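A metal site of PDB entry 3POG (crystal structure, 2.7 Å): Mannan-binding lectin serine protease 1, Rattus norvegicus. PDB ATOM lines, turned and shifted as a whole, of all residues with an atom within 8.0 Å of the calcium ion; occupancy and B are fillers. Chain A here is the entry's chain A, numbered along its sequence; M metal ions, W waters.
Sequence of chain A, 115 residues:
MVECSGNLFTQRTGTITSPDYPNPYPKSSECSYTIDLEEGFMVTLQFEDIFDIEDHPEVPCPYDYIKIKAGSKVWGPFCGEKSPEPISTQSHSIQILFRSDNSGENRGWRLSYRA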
ATOM      1  N   TYR A  25      -8.220   1.554 -14.559  1.00  0.00           N
ATOM      2  CA  TYR A  25      -9.491   1.062 -15.107  1.00  0.00           C
ATOM      3  C   TYR A  25      -9.815  -0.291 -14.516  1.00  0.00           C
ATOM      4  O   TYR A  25      -8.894  -1.028 -14.190  1.00  0.00           O
ATOM      5  CB  TYR A  25      -9.441   0.952 -16.630  1.00  0.00           C
ATOM      6  CG  TYR A  25      -8.228   0.253 -17.238  1.00  0.00           C
ATOM      7  CD1 TYR A  25      -8.091  -1.138 -17.214  1.00  0.00           C
ATOM      8  CD2 TYR A  25      -7.257   0.987 -17.903  1.00  0.00           C
ATOM      9  CE1 TYR A  25      -7.011  -1.765 -17.804  1.00  0.00           C
ATOM     10  CE2 TYR A  25      -6.165   0.355 -18.500  1.00  0.00           C
ATOM     11  CZ  TYR A  25      -6.065  -1.004 -18.440  1.00  0.00           C
ATOM     12  OH  TYR A  25      -4.978  -1.589 -19.016  1.00  0.00           O
ATOM     13  N   PRO A  26     -11.099  -0.622 -14.373  1.00  0.00           N
ATOM     14  CA  PRO A  26     -11.437  -1.827 -13.649  1.00  0.00           C
ATOM     15  C   PRO A  26     -11.095  -3.048 -14.468  1.00  0.00           C
ATOM     16  O   PRO A  26     -11.019  -2.965 -15.710  1.00  0.00           O
ATOM     17  CB  PRO A  26     -12.958  -1.726 -13.476  1.00  0.00           C
ATOM     18  CG  PRO A  26     -13.334  -0.358 -13.894  1.00  0.00           C
ATOM     19  CD  PRO A  26     -12.308   0.066 -14.861  1.00  0.00           C
ATOM     20  N   LYS A  27     -10.871  -4.175 -13.769  1.00  0.00           N
ATOM     21  CA  LYS A  27     -10.566  -5.470 -14.406  1.00  0.00           C
ATOM     22  C   LYS A  27     -11.809  -6.205 -14.907  1.00  0.00           C
ATOM     23  O   LYS A  27     -12.934  -5.865 -14.538  1.00  0.00           O
ATOM     24  CB  LYS A  27      -9.720  -6.368 -13.513  1.00  0.00           C
ATOM     25  CG  LYS A  27     -10.125  -6.363 -12.050  1.00  0.00           C
ATOM     26  CD  LYS A  27      -9.986  -7.744 -11.423  1.00  0.00           C
ATOM     27  CE  LYS A  27     -10.274  -7.677  -9.930  1.00  0.00           C
ATOM     28  NZ  LYS A  27      -9.888  -8.901  -9.286  1.00  0.00           N
ATOM     29  N   SER A  28     -11.569  -7.232 -15.719  1.00  0.00           N
ATOM     30  CA  SER A  28     -12.545  -7.899 -16.596  1.00  0.00           C
ATOM     31  C   SER A  28     -13.656  -6.979 -17.125  1.00  0.00           C
ATOM     32  O   SER A  28     -14.822  -7.114 -16.769  1.00  0.00           O
ATOM     33  CB  SER A  28     -13.077  -9.127 -15.896  1.00  0.00           C
ATOM     34  OG  SER A  28     -12.005  -9.695 -15.174  1.00  0.00           O
ATOM     35  N   ILE A  53      -2.221   1.543 -21.320  1.00  0.00           N
ATOM     36  CA  ILE A  53      -2.934   0.260 -21.408  1.00  0.00           C
ATOM     37  C   ILE A  53      -1.914  -0.870 -21.324  1.00  0.00           C
ATOM     38  O   ILE A  53      -0.832  -0.799 -21.924  1.00  0.00           O
ATOM     39  CB  ILE A  53      -3.774   0.093 -22.713  1.00  0.00           C
ATOM     40  CG1 ILE A  53      -4.791   1.222 -22.865  1.00  0.00           C
ATOM     41  CG2 ILE A  53      -4.514  -1.198 -22.690  1.00  0.00           C
ATOM     42  CD1 ILE A  53      -5.678   1.070 -24.005  1.00  0.00           C
ATOM     43  N   GLU A  54      -2.248  -1.916 -20.593  1.00  0.00           N
ATOM     44  CA  GLU A  54      -1.301  -2.994 -20.373  1.00  0.00           C
ATOM     45  C   GLU A  54      -0.850  -3.628 -21.681  1.00  0.00           C
ATOM     46  O   GLU A  54      -1.636  -3.767 -22.605  1.00  0.00           O
ATOM     47  CB  GLU A  54      -1.863  -4.014 -19.395  1.00  0.00           C
ATOM     48  CG  GLU A  54      -0.831  -4.969 -18.893  1.00  0.00           C
ATOM     49  CD  GLU A  54      -1.414  -6.045 -18.067  1.00  0.00           C
ATOM     50  OE1 GLU A  54      -2.675  -6.159 -18.032  1.00  0.00           O
ATOM     51  OE2 GLU A  54      -0.611  -6.772 -17.442  1.00  0.00           O
ATOM     52  N   ASP A  55       0.400  -4.065 -21.686  1.00  0.00           N
ATOM     53  CA  ASP A  55       1.215  -4.247 -22.878  1.00  0.00           C
ATOM     54  C   ASP A  55       2.092  -5.475 -22.604  1.00  0.00           C
ATOM     55  O   ASP A  55       1.992  -6.111 -21.535  1.00  0.00           O
ATOM     56  CB  ASP A  55       2.091  -3.010 -23.018  1.00  0.00           C
ATOM     57  CG  ASP A  55       3.001  -3.032 -24.224  1.00  0.00           C
ATOM     58  OD1 ASP A  55       4.077  -2.391 -24.109  1.00  0.00           O
ATOM     59  OD2 ASP A  55       2.644  -3.657 -25.290  1.00  0.00           O
ATOM     60  N   PRO A  62      -1.786  -8.556 -25.971  1.00  0.00           N
ATOM     61  CA  PRO A  62      -2.702  -9.442 -25.304  1.00  0.00           C
ATOM     62  C   PRO A  62      -3.324  -8.686 -24.123  1.00  0.00           C
ATOM     63  O   PRO A  62      -3.126  -7.451 -23.979  1.00  0.00           O
ATOM     64  CB  PRO A  62      -1.785 -10.571 -24.812  1.00  0.00           C
ATOM     65  CG  PRO A  62      -0.405  -9.993 -24.752  1.00  0.00           C
ATOM     66  CD  PRO A  62      -0.416  -8.643 -25.435  1.00  0.00           C
ATOM     67  N   TYR A  63      -4.058  -9.385 -23.258  1.00  0.00           N
ATOM     68  CA  TYR A  63      -4.580  -8.756 -22.057  1.00  0.00           C
ATOM     69  C   TYR A  63      -5.570  -7.662 -22.365  1.00  0.00           C
ATOM     70  O   TYR A  63      -6.750  -7.917 -22.576  1.00  0.00           O
ATOM     71  CB  TYR A  63      -3.496  -8.138 -21.183  1.00  0.00           C
ATOM     72  CG  TYR A  63      -2.242  -8.914 -21.029  1.00  0.00           C
ATOM     73  CD1 TYR A  63      -2.229 -10.306 -21.103  1.00  0.00           C
ATOM     74  CD2 TYR A  63      -1.045  -8.264 -20.826  1.00  0.00           C
ATOM     75  CE1 TYR A  63      -1.040 -11.022 -20.968  1.00  0.00           C
ATOM     76  CE2 TYR A  63       0.142  -8.942 -20.705  1.00  0.00           C
ATOM     77  CZ  TYR A  63       0.137 -10.318 -20.761  1.00  0.00           C
ATOM     78  OH  TYR A  63       1.329 -10.965 -20.607  1.00  0.00           O
ATOM     79  N   ASP A  64      -5.091  -6.430 -22.388  1.00  0.00           N
ATOM     80  CA  ASP A  64      -5.967  -5.294 -22.384  1.00  0.00           C
ATOM     81  C   ASP A  64      -5.829  -4.631 -23.738  1.00  0.00           C
ATOM     82  O   ASP A  64      -4.871  -4.904 -24.464  1.00  0.00           O
ATOM     83  CB  ASP A  64      -5.577  -4.410 -21.191  1.00  0.00           C
ATOM     84  CG  ASP A  64      -5.559  -5.189 -19.877  1.00  0.00           C
ATOM     85  OD1 ASP A  64      -6.050  -6.343 -19.853  1.00  0.00           O
ATOM     86  OD2 ASP A  64      -5.077  -4.693 -18.837  1.00  0.00           O
ATOM     87  N   TYR A  65      -6.795  -3.810 -24.124  1.00  0.00           N
ATOM     88  CA  TYR A  65      -6.702  -3.144 -25.409  1.00  0.00           C
ATOM     89  C   TYR A  65      -7.880  -2.251 -25.795  1.00  0.00           C
ATOM     90  O   TYR A  65      -9.025  -2.572 -25.520  1.00  0.00           O
ATOM     91  CB  TYR A  65      -6.481  -4.165 -26.517  1.00  0.00           C
ATOM     92  CG  TYR A  65      -7.677  -5.018 -26.885  1.00  0.00           C
ATOM     93  CD1 TYR A  65      -8.749  -4.480 -27.604  1.00  0.00           C
ATOM     94  CD2 TYR A  65      -7.721  -6.378 -26.566  1.00  0.00           C
ATOM     95  CE1 TYR A  65      -9.820  -5.252 -27.957  1.00  0.00           C
ATOM     96  CE2 TYR A  65      -8.790  -7.164 -26.922  1.00  0.00           C
ATOM     97  CZ  TYR A  65      -9.842  -6.597 -27.623  1.00  0.00           C
ATOM     98  OH  TYR A  65     -10.910  -7.378 -27.965  1.00  0.00           O
ATOM     99  N   PHE A  98     -13.192  -0.976 -25.694  1.00  0.00           N
ATOM    100  CA  PHE A  98     -12.053  -1.113 -24.807  1.00  0.00           C
ATOM    101  C   PHE A  98     -12.263  -2.340 -23.975  1.00  0.00           C
ATOM    102  O   PHE A  98     -13.390  -2.595 -23.560  1.00  0.00           O
ATOM    103  CB  PHE A  98     -11.905   0.127 -23.903  1.00  0.00           C
ATOM    104  CG  PHE A  98     -10.977  -0.067 -22.701  1.00  0.00           C
ATOM    105  CD1 PHE A  98      -9.627  -0.417 -22.875  1.00  0.00           C
ATOM    106  CD2 PHE A  98     -11.443   0.104 -21.411  1.00  0.00           C
ATOM    107  CE1 PHE A  98      -8.780  -0.596 -21.779  1.00  0.00           C
ATOM    108  CE2 PHE A  98     -10.595  -0.070 -20.303  1.00  0.00           C
ATOM    109  CZ  PHE A  98      -9.264  -0.414 -20.486  1.00  0.00           C
ATOM    110  N   ARG A  99     -11.182  -3.088 -23.708  1.00  0.00           N
ATOM    111  CA  ARG A  99     -11.255  -4.393 -23.021  1.00  0.00           C
ATOM    112  C   ARG A  99     -10.059  -4.692 -22.121  1.00  0.00           C
ATOM    113  O   ARG A  99      -8.936  -4.727 -22.576  1.00  0.00           O
ATOM    114  CB  ARG A  99     -11.371  -5.504 -24.060  1.00  0.00           C
ATOM    115  CG  ARG A  99     -12.772  -5.928 -24.520  1.00  0.00           C
ATOM    116  CD  ARG A  99     -13.045  -7.321 -23.947  1.00  0.00           C
ATOM    117  NE  ARG A  99     -11.783  -8.022 -23.632  1.00  0.00           N
ATOM    118  CZ  ARG A  99     -11.496  -9.275 -24.026  1.00  0.00           C
ATOM    119  NH1 ARG A  99     -10.309  -9.825 -23.689  1.00  0.00           N
ATOM    120  NH2 ARG A  99     -12.392  -9.988 -24.746  1.00  0.00           N
ATOM    121  N   SER A 100     -10.310  -4.973 -20.846  1.00  0.00           N
ATOM    122  CA  SER A 100      -9.257  -5.365 -19.939  1.00  0.00           C
ATOM    123  C   SER A 100      -9.487  -6.755 -19.355  1.00  0.00           C
ATOM    124  O   SER A 100     -10.624  -7.148 -19.151  1.00  0.00           O
ATOM    125  CB  SER A 100      -9.169  -4.358 -18.790  1.00  0.00           C
ATOM    126  OG  SER A 100     -10.416  -4.160 -18.163  1.00  0.00           O
ATOM    127  N   ASP A 101      -8.402  -7.477 -19.067  1.00  0.00           N
ATOM    128  CA  ASP A 101      -8.448  -8.764 -18.373  1.00  0.00           C
ATOM    129  C   ASP A 101      -8.550  -8.569 -16.880  1.00  0.00           C
ATOM    130  O   ASP A 101      -9.003  -7.524 -16.427  1.00  0.00           O
ATOM    131  CB  ASP A 101      -7.191  -9.581 -18.689  1.00  0.00           C
ATOM    132  CG  ASP A 101      -5.921  -8.881 -18.297  1.00  0.00           C
ATOM    133  OD1 ASP A 101      -5.974  -7.664 -17.964  1.00  0.00           O
ATOM    134  OD2 ASP A 101      -4.852  -9.527 -18.333  1.00  0.00           O
ATOM    135  N   ASN A 102      -8.072  -9.548 -16.116  1.00  0.00           N
ATOM    136  CA  ASN A 102      -8.386  -9.698 -14.690  1.00  0.00           C
ATOM    137  C   ASN A 102      -7.278  -9.217 -13.757  1.00  0.00           C
ATOM    138  O   ASN A 102      -7.295  -9.533 -12.588  1.00  0.00           O
ATOM    139  CB  ASN A 102      -8.624 -11.184 -14.387  1.00  0.00           C
ATOM    140  CG  ASN A 102      -9.645 -11.422 -13.280  1.00  0.00           C
ATOM    141  OD1 ASN A 102      -9.319 -11.945 -12.181  1.00  0.00           O
ATOM    142  ND2 ASN A 102     -10.914 -11.083 -13.562  1.00  0.00           N
ATOM    143  N   SER A 103      -6.310  -8.472 -14.282  1.00  0.00           N
ATOM    144  CA  SER A 103      -5.193  -7.961 -13.475  1.00  0.00           C
ATOM    145  C   SER A 103      -4.564  -6.773 -14.157  1.00  0.00           C
ATOM    146  O   SER A 103      -4.866  -6.495 -15.293  1.00  0.00           O
ATOM    147  CB  SER A 103      -4.115  -9.044 -13.246  1.00  0.00           C
ATOM    148  OG  SER A 103      -3.483  -9.446 -14.449  1.00  0.00           O
ATOM    149  N   GLY A 104      -3.669  -6.101 -13.459  1.00  0.00           N
ATOM    150  CA  GLY A 104      -2.902  -5.009 -14.060  1.00  0.00           C
ATOM    151  C   GLY A 104      -3.122  -3.722 -13.311  1.00  0.00           C
ATOM    152  O   GLY A 104      -4.121  -3.580 -12.616  1.00  0.00           O
ATOM    153  N   GLU A 105      -2.174  -2.787 -13.408  1.00  0.00           N
ATOM    154  CA  GLU A 105      -2.419  -1.474 -12.827  1.00  0.00           C
ATOM    155  C   GLU A 105      -2.114  -0.407 -13.868  1.00  0.00           C
ATOM    156  O   GLU A 105      -1.158   0.313 -13.761  1.00  0.00           O
ATOM    157  CB  GLU A 105      -1.638  -1.260 -11.507  1.00  0.00           C
ATOM    158  CG  GLU A 105      -2.398  -0.388 -10.484  1.00  0.00           C
ATOM    159  CD  GLU A 105      -1.572  -0.015  -9.250  1.00  0.00           C
ATOM    160  OE1 GLU A 105      -0.939   1.071  -9.218  1.00  0.00           O
ATOM    161  OE2 GLU A 105      -1.562  -0.791  -8.286  1.00  0.00           O
ATOM    162  N   ASN A 106      -2.938  -0.316 -14.893  1.00  0.00           N
ATOM    163  CA  ASN A 106      -2.800   0.772 -15.818  1.00  0.00           C
ATOM    164  C   ASN A 106      -3.917   1.793 -15.772  1.00  0.00           C
ATOM    165  O   ASN A 106      -5.089   1.462 -15.537  1.00  0.00           O
ATOM    166  CB  ASN A 106      -2.550   0.254 -17.212  1.00  0.00           C
ATOM    167  CG  ASN A 106      -1.543  -0.861 -17.224  1.00  0.00           C
ATOM    168  OD1 ASN A 106      -1.751  -1.897 -16.610  1.00  0.00           O
ATOM    169  ND2 ASN A 106      -0.436  -0.660 -17.928  1.00  0.00           N
HETATM  170 CA    CA M   1      -5.099  -5.799 -17.222  1.00  0.00          CA
HETATM  171  O   HOH W   1      -4.241  -3.334 -16.397  1.00  0.00           O
HETATM  172  O   HOH W   2      -7.200  -4.908 -15.906  1.00  0.00           O
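CA of Gly 104 touches the calcium ion, 3.9 Å away.
Within 4 Å of the calcium ion: Glu 54, Asp 64, Asp 101, Ser 103 and Gly 104.
Water W1 lies within hydrogen-bond range of OD1 of Asn 106 (2.9 Å) and OH of Tyr 25 (3.2 Å).
The calcium ion is bound by the side-chain carboxylate (OD2) of Asp 64 (2.0 Å), the backbone carbonyl oxygen (O) of Ser 103 (2.1 Å), the side-chain carboxylate (OD1) of Asp 101 (2.2 Å), the side-chain carboxylate (OE1) of Glu 54 (2.6 Å), water W2 (2.6 Å), water W1 (2.7 Å) and the side-chain carboxylate (OD1) of Asp 64 (2.8 Å).
The calcium ion has seven donor atoms within binding distance.
The backbone carbonyl oxygen (O) of Asp 101 is in hydrogen-bond range of the backbone NH (N) of Ser 28, at 2.7 Å.
The backbone NH (N) of Glu 54 is in hydrogen-bond range of the side-chain hydroxyl (OH) of Tyr 25 (3.2 Å).
The backbone NH (N) of Glu 54 lies close to the side-chain amide nitrogen (ND2) of Asn 106 (3.5 Å).
OD2 of Asp 64 sits close to OH of Tyr 25 (3.1 Å).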
